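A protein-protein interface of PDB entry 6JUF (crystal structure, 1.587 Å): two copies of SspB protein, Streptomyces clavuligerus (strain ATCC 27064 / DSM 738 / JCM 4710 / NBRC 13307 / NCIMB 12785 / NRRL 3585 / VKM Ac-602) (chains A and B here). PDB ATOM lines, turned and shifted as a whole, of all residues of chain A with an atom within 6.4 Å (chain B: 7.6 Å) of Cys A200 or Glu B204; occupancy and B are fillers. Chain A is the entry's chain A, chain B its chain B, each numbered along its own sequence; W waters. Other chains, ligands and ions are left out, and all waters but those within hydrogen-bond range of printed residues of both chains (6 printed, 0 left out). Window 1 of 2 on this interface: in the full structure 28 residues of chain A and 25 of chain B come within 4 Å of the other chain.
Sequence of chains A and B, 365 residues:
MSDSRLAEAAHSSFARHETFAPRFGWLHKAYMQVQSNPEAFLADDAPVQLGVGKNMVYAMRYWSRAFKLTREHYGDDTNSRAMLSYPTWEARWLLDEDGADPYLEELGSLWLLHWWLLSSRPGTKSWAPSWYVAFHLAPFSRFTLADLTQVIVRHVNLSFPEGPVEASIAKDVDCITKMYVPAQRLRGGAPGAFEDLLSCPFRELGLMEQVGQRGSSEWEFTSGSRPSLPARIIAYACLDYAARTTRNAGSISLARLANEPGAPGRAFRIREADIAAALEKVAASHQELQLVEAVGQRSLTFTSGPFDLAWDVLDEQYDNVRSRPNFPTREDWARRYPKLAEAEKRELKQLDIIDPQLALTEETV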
ATOM      1  N   ALA A  21       5.090  16.766  30.013  1.00  0.00           N
ATOM      2  CA  ALA A  21       4.086  15.702  30.199  1.00  0.00           C
ATOM      3  C   ALA A  21       4.090  14.815  28.977  1.00  0.00           C
ATOM      4  O   ALA A  21       4.657  15.190  27.950  1.00  0.00           O
ATOM      5  CB  ALA A  21       2.729  16.322  30.474  1.00  0.00           C
ATOM      6  N   PRO A  22       3.489  13.612  29.061  1.00  0.00           N
ATOM      7  CA  PRO A  22       3.586  12.690  27.909  1.00  0.00           C
ATOM      8  C   PRO A  22       2.930  13.260  26.639  1.00  0.00           C
ATOM      9  O   PRO A  22       1.960  14.002  26.727  1.00  0.00           O
ATOM     10  CB  PRO A  22       2.820  11.428  28.396  1.00  0.00           C
ATOM     11  CG  PRO A  22       2.886  11.522  29.905  1.00  0.00           C
ATOM     12  CD  PRO A  22       2.856  12.977  30.231  1.00  0.00           C
ATOM     13  N   ARG A  23       3.437  12.898  25.491  1.00  0.00           N
ATOM     14  CA  ARG A  23       2.835  13.226  24.223  1.00  0.00           C
ATOM     15  C   ARG A  23       2.646  11.962  23.396  1.00  0.00           C
ATOM     16  O   ARG A  23       3.511  11.067  23.441  1.00  0.00           O
ATOM     17  CB  ARG A  23       3.817  14.115  23.414  1.00  0.00           C
ATOM     18  CG  ARG A  23       4.313  15.362  24.146  1.00  0.00           C
ATOM     19  CD  ARG A  23       4.950  16.371  23.184  1.00  0.00           C
ATOM     20  NE  ARG A  23       5.690  17.351  23.968  1.00  0.00           N
ATOM     21  CZ  ARG A  23       6.355  18.363  23.436  1.00  0.00           C
ATOM     22  NH1 ARG A  23       6.408  18.465  22.093  1.00  0.00           N
ATOM     23  NH2 ARG A  23       7.039  19.209  24.213  1.00  0.00           N
ATOM     24  N   LYS A 178      -0.007  19.037  34.807  1.00  0.00           N
ATOM     25  CA  LYS A 178      -0.115  19.215  33.356  1.00  0.00           C
ATOM     26  C   LYS A 178      -0.627  17.948  32.654  1.00  0.00           C
ATOM     27  O   LYS A 178      -1.306  18.057  31.617  1.00  0.00           O
ATOM     28  CB  LYS A 178       1.288  19.593  32.749  1.00  0.00           C
ATOM     29  CG  LYS A 178       1.638  21.033  33.060  1.00  0.00           C
ATOM     30  CD  LYS A 178       2.799  21.530  32.220  1.00  0.00           C
ATOM     31  CE  LYS A 178       4.102  21.191  32.844  1.00  0.00           C
ATOM     32  NZ  LYS A 178       5.141  21.648  31.892  1.00  0.00           N
ATOM     33  N   MET A 179      -0.336  16.779  33.223  1.00  0.00           N
ATOM     34  CA  MET A 179      -0.691  15.508  32.595  1.00  0.00           C
ATOM     35  C   MET A 179      -2.200  15.243  32.764  1.00  0.00           C
ATOM     36  O   MET A 179      -2.843  14.653  31.877  1.00  0.00           O
ATOM     37  CB  MET A 179       0.114  14.359  33.249  1.00  0.00           C
ATOM     38  CG  MET A 179      -0.299  12.945  32.756  1.00  0.00           C
ATOM     39  SD  MET A 179       1.042  11.812  33.240  1.00  0.00           S
ATOM     40  CE  MET A 179       0.294  10.297  32.672  1.00  0.00           C
ATOM     41  N   TYR A 180      -2.751  15.595  33.939  1.00  0.00           N
ATOM     42  CA  TYR A 180      -4.121  15.166  34.252  1.00  0.00           C
ATOM     43  C   TYR A 180      -5.236  16.225  34.274  1.00  0.00           C
ATOM     44  O   TYR A 180      -6.415  15.850  34.232  1.00  0.00           O
ATOM     45  CB  TYR A 180      -4.169  14.426  35.615  1.00  0.00           C
ATOM     46  CG  TYR A 180      -3.350  13.140  35.652  1.00  0.00           C
ATOM     47  CD1 TYR A 180      -3.820  11.973  34.978  1.00  0.00           C
ATOM     48  CD2 TYR A 180      -2.128  13.067  36.306  1.00  0.00           C
ATOM     49  CE1 TYR A 180      -3.038  10.797  34.975  1.00  0.00           C
ATOM     50  CE2 TYR A 180      -1.375  11.910  36.296  1.00  0.00           C
ATOM     51  CZ  TYR A 180      -1.824  10.771  35.656  1.00  0.00           C
ATOM     52  OH  TYR A 180      -1.065   9.630  35.697  1.00  0.00           O
ATOM     53  N   VAL A 181      -4.920  17.516  34.442  1.00  0.00           N
ATOM     54  CA  VAL A 181      -5.949  18.547  34.588  1.00  0.00           C
ATOM     55  C   VAL A 181      -6.298  19.164  33.212  1.00  0.00           C
ATOM     56  O   VAL A 181      -5.501  19.110  32.260  1.00  0.00           O
ATOM     57  CB  VAL A 181      -5.559  19.698  35.590  1.00  0.00           C
ATOM     58  CG1 VAL A 181      -5.097  19.110  36.910  1.00  0.00           C
ATOM     59  CG2 VAL A 181      -4.532  20.655  34.992  1.00  0.00           C
ATOM     60  N   PRO A 182      -7.519  19.719  33.096  1.00  0.00           N
ATOM     61  CA  PRO A 182      -7.881  20.327  31.803  1.00  0.00           C
ATOM     62  C   PRO A 182      -6.936  21.440  31.414  1.00  0.00           C
ATOM     63  O   PRO A 182      -6.422  22.159  32.290  1.00  0.00           O
ATOM     64  CB  PRO A 182      -9.310  20.871  32.034  1.00  0.00           C
ATOM     65  CG  PRO A 182      -9.846  20.013  33.189  1.00  0.00           C
ATOM     66  CD  PRO A 182      -8.636  19.709  34.063  1.00  0.00           C
ATOM     67  N   ALA A 183      -6.651  21.546  30.104  1.00  0.00           N
ATOM     68  CA  ALA A 183      -5.691  22.511  29.603  1.00  0.00           C
ATOM     69  C   ALA A 183      -6.055  23.945  30.032  1.00  0.00           C
ATOM     70  O   ALA A 183      -5.211  24.786  30.219  1.00  0.00           O
ATOM     71  CB  ALA A 183      -5.643  22.414  28.070  1.00  0.00           C
ATOM     72  N   GLN A 184      -7.352  24.181  30.218  1.00  0.00           N
ATOM     73  CA  GLN A 184      -7.854  25.538  30.582  1.00  0.00           C
ATOM     74  C   GLN A 184      -7.369  25.996  31.957  1.00  0.00           C
ATOM     75  O   GLN A 184      -7.291  27.214  32.202  1.00  0.00           O
ATOM     76  CB  GLN A 184      -9.385  25.531  30.548  1.00  0.00           C
ATOM     77  CG  GLN A 184      -9.944  25.427  29.127  1.00  0.00           C
ATOM     78  CD  GLN A 184      -9.617  24.126  28.367  1.00  0.00           C
ATOM     79  OE1 GLN A 184      -9.097  24.154  27.199  1.00  0.00           O
ATOM     80  NE2 GLN A 184      -9.980  22.995  28.948  1.00  0.00           N
ATOM     81  N   LEU A 198       0.841  22.297  25.397  1.00  0.00           N
ATOM     82  CA  LEU A 198       0.899  21.050  24.623  1.00  0.00           C
ATOM     83  C   LEU A 198      -0.342  20.242  24.894  1.00  0.00           C
ATOM     84  O   LEU A 198      -0.930  20.342  25.959  1.00  0.00           O
ATOM     85  CB  LEU A 198       2.154  20.240  24.959  1.00  0.00           C
ATOM     86  CG  LEU A 198       3.397  21.046  24.593  1.00  0.00           C
ATOM     87  CD1 LEU A 198       4.510  20.780  25.540  1.00  0.00           C
ATOM     88  CD2 LEU A 198       3.798  20.796  23.159  1.00  0.00           C
ATOM     89  N   SER A 199      -0.757  19.440  23.933  1.00  0.00           N
ATOM     90  CA  SER A 199      -1.792  18.461  24.214  1.00  0.00           C
ATOM     91  C   SER A 199      -1.281  17.342  25.160  1.00  0.00           C
ATOM     92  O   SER A 199      -0.074  17.071  25.231  1.00  0.00           O
ATOM     93  CB  SER A 199      -2.324  17.844  22.913  1.00  0.00           C
ATOM     94  OG  SER A 199      -1.305  17.137  22.230  1.00  0.00           O
ATOM     95  N   CYS A 200      -2.195  16.765  25.964  1.00  0.00           N
ATOM     96  CA  CYS A 200      -1.776  15.572  26.736  1.00  0.00           C
ATOM     97  C   CYS A 200      -2.996  14.686  26.821  1.00  0.00           C
ATOM     98  O   CYS A 200      -4.008  15.107  27.439  1.00  0.00           O
ATOM     99  CB  CYS A 200      -1.311  15.946  28.169  1.00  0.00           C
ATOM    100  SG  CYS A 200      -0.687  14.452  28.959  1.00  0.00           S
ATOM    101  N   PRO A 201      -2.955  13.516  26.190  1.00  0.00           N
ATOM    102  CA  PRO A 201      -4.206  12.737  26.052  1.00  0.00           C
ATOM    103  C   PRO A 201      -4.718  12.200  27.387  1.00  0.00           C
ATOM    104  O   PRO A 201      -5.871  11.799  27.499  1.00  0.00           O
ATOM    105  CB  PRO A 201      -3.823  11.601  25.081  1.00  0.00           C
ATOM    106  CG  PRO A 201      -2.309  11.467  25.244  1.00  0.00           C
ATOM    107  CD  PRO A 201      -1.808  12.877  25.484  1.00  0.00           C
ATOM    108  N   PHE A 202      -3.882  12.248  28.417  1.00  0.00           N
ATOM    109  CA  PHE A 202      -4.336  11.786  29.728  1.00  0.00           C
ATOM    110  C   PHE A 202      -5.328  12.720  30.393  1.00  0.00           C
ATOM    111  O   PHE A 202      -6.026  12.305  31.326  1.00  0.00           O
ATOM    112  CB  PHE A 202      -3.138  11.519  30.633  1.00  0.00           C
ATOM    113  CG  PHE A 202      -2.281  10.376  30.117  1.00  0.00           C
ATOM    114  CD1 PHE A 202      -2.609   9.056  30.424  1.00  0.00           C
ATOM    115  CD2 PHE A 202      -1.249  10.616  29.196  1.00  0.00           C
ATOM    116  CE1 PHE A 202      -1.831   7.990  29.958  1.00  0.00           C
ATOM    117  CE2 PHE A 202      -0.511   9.545  28.671  1.00  0.00           C
ATOM    118  CZ  PHE A 202      -0.814   8.219  29.052  1.00  0.00           C
ATOM    119  N   ARG A 203      -5.431  13.956  29.874  1.00  0.00           N
ATOM    120  CA  ARG A 203      -6.424  14.877  30.422  1.00  0.00           C
ATOM    121  C   ARG A 203      -7.850  14.377  30.192  1.00  0.00           C
ATOM    122  O   ARG A 203      -8.773  14.719  30.955  1.00  0.00           O
ATOM    123  CB  ARG A 203      -6.225  16.295  29.879  1.00  0.00           C
ATOM    124  CG  ARG A 203      -4.872  16.875  30.196  1.00  0.00           C
ATOM    125  CD  ARG A 203      -4.636  18.160  29.410  1.00  0.00           C
ATOM    126  NE  ARG A 203      -3.271  18.640  29.733  1.00  0.00           N
ATOM    127  CZ  ARG A 203      -2.516  19.300  28.848  1.00  0.00           C
ATOM    128  NH1 ARG A 203      -3.031  19.586  27.667  1.00  0.00           N
ATOM    129  NH2 ARG A 203      -1.290  19.714  29.143  1.00  0.00           N
ATOM    130  N   GLU A 204      -8.034  13.539  29.173  1.00  0.00           N
ATOM    131  CA  GLU A 204      -9.362  13.013  28.892  1.00  0.00           C
ATOM    132  C   GLU A 204      -9.866  12.074  29.955  1.00  0.00           C
ATOM    133  O   GLU A 204     -11.075  11.810  29.972  1.00  0.00           O
ATOM    134  CB  GLU A 204      -9.437  12.279  27.535  1.00  0.00           C
ATOM    135  CG  GLU A 204      -9.311  13.243  26.399  1.00  0.00           C
ATOM    136  CD  GLU A 204     -10.174  12.813  25.221  1.00  0.00           C
ATOM    137  OE1 GLU A 204      -9.647  12.678  24.122  1.00  0.00           O
ATOM    138  OE2 GLU A 204     -11.392  12.623  25.420  1.00  0.00           O
ATOM    139  N   LEU B 104      -0.029  16.401  16.210  1.00  0.00           N
ATOM    140  CA  LEU B 104      -0.906  17.325  16.907  1.00  0.00           C
ATOM    141  C   LEU B 104      -0.479  17.410  18.407  1.00  0.00           C
ATOM    142  O   LEU B 104      -1.335  17.305  19.323  1.00  0.00           O
ATOM    143  CB  LEU B 104      -2.377  16.936  16.777  1.00  0.00           C
ATOM    144  CG  LEU B 104      -2.875  16.918  15.287  1.00  0.00           C
ATOM    145  CD1 LEU B 104      -4.383  16.664  15.282  1.00  0.00           C
ATOM    146  CD2 LEU B 104      -2.521  18.150  14.487  1.00  0.00           C
ATOM    147  N   GLU B 105       0.819  17.692  18.599  1.00  0.00           N
ATOM    148  CA  GLU B 105       1.395  17.840  19.924  1.00  0.00           C
ATOM    149  C   GLU B 105       1.071  19.150  20.596  1.00  0.00           C
ATOM    150  O   GLU B 105       1.079  19.222  21.829  1.00  0.00           O
ATOM    151  CB  GLU B 105       2.913  17.648  19.840  1.00  0.00           C
ATOM    152  CG  GLU B 105       3.299  16.220  19.516  1.00  0.00           C
ATOM    153  CD  GLU B 105       4.776  16.072  19.236  1.00  0.00           C
ATOM    154  OE1 GLU B 105       5.604  16.837  19.745  1.00  0.00           O
ATOM    155  OE2 GLU B 105       5.099  15.197  18.405  1.00  0.00           O
ATOM    156  N   LEU B 107      -1.489  22.364  21.328  1.00  0.00           N
ATOM    157  CA  LEU B 107      -2.914  22.683  21.329  1.00  0.00           C
ATOM    158  C   LEU B 107      -3.267  23.718  20.248  1.00  0.00           C
ATOM    159  O   LEU B 107      -4.356  23.652  19.651  1.00  0.00           O
ATOM    160  CB  LEU B 107      -3.454  23.049  22.708  1.00  0.00           C
ATOM    161  CG  LEU B 107      -3.559  21.831  23.619  1.00  0.00           C
ATOM    162  CD1 LEU B 107      -4.020  22.244  25.010  1.00  0.00           C
ATOM    163  CD2 LEU B 107      -4.473  20.755  23.046  1.00  0.00           C
ATOM    164  N   LEU B 110      -4.695  22.155  17.116  1.00  0.00           N
ATOM    165  CA  LEU B 110      -6.095  21.801  17.196  1.00  0.00           C
ATOM    166  C   LEU B 110      -6.972  23.049  17.019  1.00  0.00           C
ATOM    167  O   LEU B 110      -8.023  22.981  16.326  1.00  0.00           O
ATOM    168  CB  LEU B 110      -6.424  21.060  18.498  1.00  0.00           C
ATOM    169  CG  LEU B 110      -5.827  19.608  18.526  1.00  0.00           C
ATOM    170  CD1 LEU B 110      -5.612  19.139  19.964  1.00  0.00           C
ATOM    171  CD2 LEU B 110      -6.689  18.690  17.642  1.00  0.00           C
ATOM    172  N   TRP B 111      -6.598  24.179  17.610  1.00  0.00           N
ATOM    173  CA  TRP B 111      -7.302  25.427  17.346  1.00  0.00           C
ATOM    174  C   TRP B 111      -7.247  25.765  15.860  1.00  0.00           C
ATOM    175  O   TRP B 111      -8.233  26.184  15.311  1.00  0.00           O
ATOM    176  CB  TRP B 111      -6.619  26.566  18.128  1.00  0.00           C
ATOM    177  CG  TRP B 111      -7.010  26.576  19.586  1.00  0.00           C
ATOM    178  CD1 TRP B 111      -6.193  26.285  20.675  1.00  0.00           C
ATOM    179  CD2 TRP B 111      -8.307  26.928  20.150  1.00  0.00           C
ATOM    180  NE1 TRP B 111      -6.897  26.425  21.850  1.00  0.00           N
ATOM    181  CE2 TRP B 111      -8.175  26.789  21.601  1.00  0.00           C
ATOM    182  CE3 TRP B 111      -9.527  27.338  19.615  1.00  0.00           C
ATOM    183  CZ2 TRP B 111      -9.234  27.092  22.473  1.00  0.00           C
ATOM    184  CZ3 TRP B 111     -10.602  27.614  20.507  1.00  0.00           C
ATOM    185  CH2 TRP B 111     -10.431  27.494  21.907  1.00  0.00           C
ATOM    186  N   MET B 179     -17.509  15.901  19.900  1.00  0.00           N
ATOM    187  CA  MET B 179     -16.203  16.520  19.486  1.00  0.00           C
ATOM    188  C   MET B 179     -15.638  17.467  20.524  1.00  0.00           C
ATOM    189  O   MET B 179     -14.448  17.536  20.717  1.00  0.00           O
ATOM    190  CB  MET B 179     -16.434  17.199  18.153  1.00  0.00           C
ATOM    191  CG  MET B 179     -15.254  17.992  17.574  1.00  0.00           C
ATOM    192  SD  MET B 179     -15.543  18.374  15.843  1.00  0.00           S
ATOM    193  CE  MET B 179     -14.065  19.330  15.473  1.00  0.00           C
ATOM    194  N   TYR B 180     -16.530  18.201  21.194  1.00  0.00           N
ATOM    195  CA  TYR B 180     -16.059  19.355  22.007  1.00  0.00           C
ATOM    196  C   TYR B 180     -16.227  19.209  23.543  1.00  0.00           C
ATOM    197  O   TYR B 180     -15.571  19.889  24.279  1.00  0.00           O
ATOM    198  CB  TYR B 180     -16.756  20.653  21.575  1.00  0.00           C
ATOM    199  CG  TYR B 180     -16.381  21.114  20.180  1.00  0.00           C
ATOM    200  CD1 TYR B 180     -15.077  21.602  19.890  1.00  0.00           C
ATOM    201  CD2 TYR B 180     -17.299  21.049  19.148  1.00  0.00           C
ATOM    202  CE1 TYR B 180     -14.743  22.006  18.583  1.00  0.00           C
ATOM    203  CE2 TYR B 180     -16.979  21.478  17.837  1.00  0.00           C
ATOM    204  CZ  TYR B 180     -15.709  21.934  17.576  1.00  0.00           C
ATOM    205  OH  TYR B 180     -15.437  22.354  16.271  1.00  0.00           O
ATOM    206  N   VAL B 181     -17.129  18.319  23.969  1.00  0.00           N
ATOM    207  CA  VAL B 181     -17.426  18.196  25.427  1.00  0.00           C
ATOM    208  C   VAL B 181     -16.575  17.061  26.012  1.00  0.00           C
ATOM    209  O   VAL B 181     -16.324  16.099  25.307  1.00  0.00           O
ATOM    210  CB  VAL B 181     -18.934  17.890  25.608  1.00  0.00           C
ATOM    211  CG1 VAL B 181     -19.275  17.715  27.054  1.00  0.00           C
ATOM    212  CG2 VAL B 181     -19.737  19.021  25.059  1.00  0.00           C
ATOM    213  N   PRO B 182     -16.147  17.190  27.288  1.00  0.00           N
ATOM    214  CA  PRO B 182     -15.387  16.103  27.935  1.00  0.00           C
ATOM    215  C   PRO B 182     -16.115  14.780  27.894  1.00  0.00           C
ATOM    216  O   PRO B 182     -17.369  14.765  27.968  1.00  0.00           O
ATOM    217  CB  PRO B 182     -15.276  16.577  29.375  1.00  0.00           C
ATOM    218  CG  PRO B 182     -15.283  18.104  29.245  1.00  0.00           C
ATOM    219  CD  PRO B 182     -16.323  18.347  28.175  1.00  0.00           C
ATOM    220  N   CYS B 200     -11.191  12.255  21.620  1.00  0.00           N
ATOM    221  CA  CYS B 200     -11.327  13.233  20.558  1.00  0.00           C
ATOM    222  C   CYS B 200     -10.487  14.469  20.992  1.00  0.00           C
ATOM    223  O   CYS B 200     -10.852  15.124  21.977  1.00  0.00           O
ATOM    224  CB  CYS B 200     -12.787  13.667  20.346  1.00  0.00           C
ATOM    225  SG  CYS B 200     -12.897  14.795  18.914  1.00  0.00           S
ATOM    226  N   PRO B 201      -9.397  14.772  20.273  1.00  0.00           N
ATOM    227  CA  PRO B 201      -8.459  15.790  20.786  1.00  0.00           C
ATOM    228  C   PRO B 201      -9.027  17.198  20.820  1.00  0.00           C
ATOM    229  O   PRO B 201      -8.476  18.076  21.485  1.00  0.00           O
ATOM    230  CB  PRO B 201      -7.275  15.701  19.832  1.00  0.00           C
ATOM    231  CG  PRO B 201      -7.832  15.075  18.574  1.00  0.00           C
ATOM    232  CD  PRO B 201      -8.952  14.166  18.986  1.00  0.00           C
ATOM    233  N   PHE B 202     -10.162  17.398  20.123  1.00  0.00           N
ATOM    234  CA  PHE B 202     -10.816  18.723  20.138  1.00  0.00           C
ATOM    235  C   PHE B 202     -11.458  19.045  21.488  1.00  0.00           C
ATOM    236  O   PHE B 202     -11.763  20.216  21.786  1.00  0.00           O
ATOM    237  CB  PHE B 202     -11.828  18.854  18.970  1.00  0.00           C
ATOM    238  CG  PHE B 202     -11.141  18.867  17.627  1.00  0.00           C
ATOM    239  CD1 PHE B 202     -10.617  20.067  17.126  1.00  0.00           C
ATOM    240  CD2 PHE B 202     -10.930  17.663  16.924  1.00  0.00           C
ATOM    241  CE1 PHE B 202      -9.887  20.066  15.918  1.00  0.00           C
ATOM    242  CE2 PHE B 202     -10.195  17.677  15.710  1.00  0.00           C
ATOM    243  CZ  PHE B 202      -9.730  18.887  15.194  1.00  0.00           C
ATOM    244  N   ARG B 203     -11.656  18.022  22.313  1.00  0.00           N
ATOM    245  CA  ARG B 203     -12.149  18.282  23.720  1.00  0.00           C
ATOM    246  C   ARG B 203     -11.163  19.092  24.530  1.00  0.00           C
ATOM    247  O   ARG B 203     -11.593  19.776  25.448  1.00  0.00           O
ATOM    248  CB  ARG B 203     -12.466  16.974  24.429  1.00  0.00           C
ATOM    249  CG  ARG B 203     -13.619  16.205  23.788  1.00  0.00           C
ATOM    250  CD  ARG B 203     -13.644  14.737  24.259  1.00  0.00           C
ATOM    251  NE  ARG B 203     -14.650  14.000  23.476  1.00  0.00           N
ATOM    252  CZ  ARG B 203     -14.580  12.658  23.345  1.00  0.00           C
ATOM    253  NH1 ARG B 203     -13.682  11.948  24.006  1.00  0.00           N
ATOM    254  NH2 ARG B 203     -15.508  12.057  22.575  1.00  0.00           N
ATOM    255  N   GLU B 204      -9.891  19.067  24.141  1.00  0.00           N
ATOM    256  CA  GLU B 204      -8.866  19.861  24.832  1.00  0.00           C
ATOM    257  C   GLU B 204      -9.058  21.364  24.675  1.00  0.00           C
ATOM    258  O   GLU B 204      -8.465  22.128  25.432  1.00  0.00           O
ATOM    259  CB  GLU B 204      -7.475  19.499  24.330  1.00  0.00           C
ATOM    260  CG  GLU B 204      -7.078  18.102  24.844  1.00  0.00           C
ATOM    261  CD  GLU B 204      -5.701  18.123  25.478  1.00  0.00           C
ATOM    262  OE1 GLU B 204      -4.841  17.313  25.124  1.00  0.00           O
ATOM    263  OE2 GLU B 204      -5.509  18.947  26.390  1.00  0.00           O
ATOM    264  N   LEU B 205      -9.833  21.778  23.666  1.00  0.00           N
ATOM    265  CA  LEU B 205     -10.089  23.201  23.465  1.00  0.00           C
ATOM    266  C   LEU B 205     -11.021  23.833  24.491  1.00  0.00           C
ATOM    267  O   LEU B 205     -11.078  25.042  24.607  1.00  0.00           O
ATOM    268  CB  LEU B 205     -10.674  23.458  22.057  1.00  0.00           C
ATOM    269  CG  LEU B 205      -9.702  23.495  20.864  1.00  0.00           C
ATOM    270  CD1 LEU B 205      -8.211  23.250  21.041  1.00  0.00           C
ATOM    271  CD2 LEU B 205     -10.281  23.174  19.524  1.00  0.00           C
ATOM    272  N   GLY B 206     -11.774  22.995  25.201  1.00  0.00           N
ATOM    273  CA  GLY B 206     -12.640  23.480  26.269  1.00  0.00           C
ATOM    274  C   GLY B 206     -13.713  24.443  25.811  1.00  0.00           C
ATOM    275  O   GLY B 206     -14.109  25.368  26.523  1.00  0.00           O
ATOM    276  N   LEU B 207     -14.234  24.182  24.621  1.00  0.00           N
ATOM    277  CA  LEU B 207     -15.202  25.054  24.010  1.00  0.00           C
ATOM    278  C   LEU B 207     -16.670  24.832  24.433  1.00  0.00           C
ATOM    279  O   LEU B 207     -17.493  25.729  24.238  1.00  0.00           O
ATOM    280  CB  LEU B 207     -15.110  24.935  22.472  1.00  0.00           C
ATOM    281  CG  LEU B 207     -13.944  25.756  21.904  1.00  0.00           C
ATOM    282  CD1 LEU B 207     -13.760  25.385  20.421  1.00  0.00           C
ATOM    283  CD2 LEU B 207     -14.167  27.245  22.050  1.00  0.00           C
ATOM    284  N   SER B 228      -4.760  28.025  26.120  1.00  0.00           N
ATOM    285  CA  SER B 228      -4.207  27.084  25.164  1.00  0.00           C
ATOM    286  C   SER B 228      -4.194  27.587  23.719  1.00  0.00           C
ATOM    287  O   SER B 228      -3.609  26.912  22.833  1.00  0.00           O
ATOM    288  CB  SER B 228      -4.938  25.728  25.195  1.00  0.00           C
ATOM    289  OG  SER B 228      -6.226  25.821  24.555  1.00  0.00           O
HETATM  290  O   HOH W   1      -7.568  19.549  28.219  1.00  0.00           O
HETATM  291  O   HOH W   2       1.544  16.722  23.107  1.00  0.00           O
HETATM  292  O   HOH W   3      -7.878  27.083  26.639  1.00  0.00           O
HETATM  293  O   HOH W   4      -6.749  15.185  26.544  1.00  0.00           O
HETATM  294  O   HOH W   5      -3.600  15.846  20.192  1.00  0.00           O
HETATM  295  O   HOH W   6     -10.291  20.384  27.999  1.00  0.00           O
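CB of Ala A183 touches CD1 of Leu B107, 3.5 Å away.
CB of Ala A183 touches OE2 of Glu B204, at 3.9 Å.
Gln A184 touches Gly B206.
Glu B105 touches Leu A198 (O to CA, 3.3 Å).
O of Leu A198 touches CD1 of Leu B107, 3.8 Å away.
CD2 of Leu B107 touches CB of Ser A199, 3.6 Å away.
Glu B204 touches Ser A199.
Arg A203 touches Leu B107 (NH1 to CD1, 3.9 Å).
The backbone NH of Arg B203 sits at hydrogen-bond distance from the backbone carbonyl oxygen of Met B179 (3.3 Å).
O of Val B181 lies close to NE of Arg B203 (3.2 Å).
The backbone carbonyl oxygen (O) of Met A179 is in hydrogen-bond range of the backbone NH (N) of Arg A203, 3.3 Å away.
SG of Cys A200 sits at hydrogen-bond distance from O of Pro A22, 3.5 Å away.
Water W2 bridges the backbone carbonyl oxygen (O) of Ser A199 (2.7 Å) and the backbone carbonyl oxygen (O) of Glu B105 (2.8 Å).
Water W1 lies within hydrogen-bond range of OE2 of Glu B204 (2.8 Å) and N of Ala A183 (2.9 Å).
Water W5 lies within hydrogen-bond range of the backbone carbonyl oxygen of Leu B104 (2.8 Å) and the side-chain hydroxyl of Ser A199 (3.3 Å).
Water W3 bridges OG of Ser B228 and OE1 of Gln A184.
Cys A200 touches just one residue of chain B: Glu B204 (2.8 Å).
Printed residues of chain B within 4 Å of Gln A184: Glu B204 (2.8 Å), Leu B205 (3.3 Å) and Gly B206 (3.5 Å).
Of the printed residues of chain B, Leu A198 touches Glu B105 and Leu B107.
Printed residues of chain B within 4 Å of Arg A23: Glu B105.
The nearest residue of chain B that does not touch Cys A200 is Leu B107 (5.4 Å).
The nearest residue of chain A that does not touch Glu B204 is Pro A201 (4.4 Å).
The nearest printed residue of chain B that does not touch Glu A204 is Pro B201 (4.4 Å).
Of the 18 printed residues of chain B, 8 touch a printed residue of chain A.
Printed residues of chain A that touch a printed residue of chain B: Arg A23, Ala A183, Gln A184, Leu A198, Ser A199, Cys A200, Arg A203 and Glu A204.
Hydrophobic or aromatic side chains of chain A that line the printed part of chain B: Ala A183 and Leu A198.
Among the printed residues, 17 pairs touch across the chains.
The backbone carbonyl oxygen of Leu B205 lies close to the side-chain amide oxygen of Gln A184 (3.4 Å).
OG of Ser A199 lies within hydrogen-bond range of O of Leu B104 (2.9 Å).
The backbone carbonyl oxygen (O) of Glu B204 sits close to the side-chain amide oxygen (OE1) of Gln A184 (2.8 Å).
The side-chain carboxylate of Glu B204 is in salt-bridge range of the guanidinium group of Arg A203 (2.9 Å).
N of Ser A199 sits at hydrogen-bond distance from O of Glu B105 (2.8 Å).
The guanidinium group (NH1) of Arg B203 is in salt-bridge range of the side-chain carboxylate (OE2) of Glu A204, at 2.8 Å.
OE1 of Glu B204 sits at hydrogen-bond distance from N of Cys A200.
OE1 of Glu B105 lies within salt-bridge range of NH1 of Arg A23 (3.0 Å).
OE1 of Glu A204 lies within hydrogen-bond range of N of Cys B200 (3.0 Å).
Cys A200 touches Glu B204, and with the chains exchanged Glu A204 touches Cys B200.
Arg A203 touches Glu B204, and with the chains exchanged Glu A204 touches Arg B203.
Of the 17 pairs that touch across the chains among the printed residues, 4 have their exchanged pair printed and touching as well.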
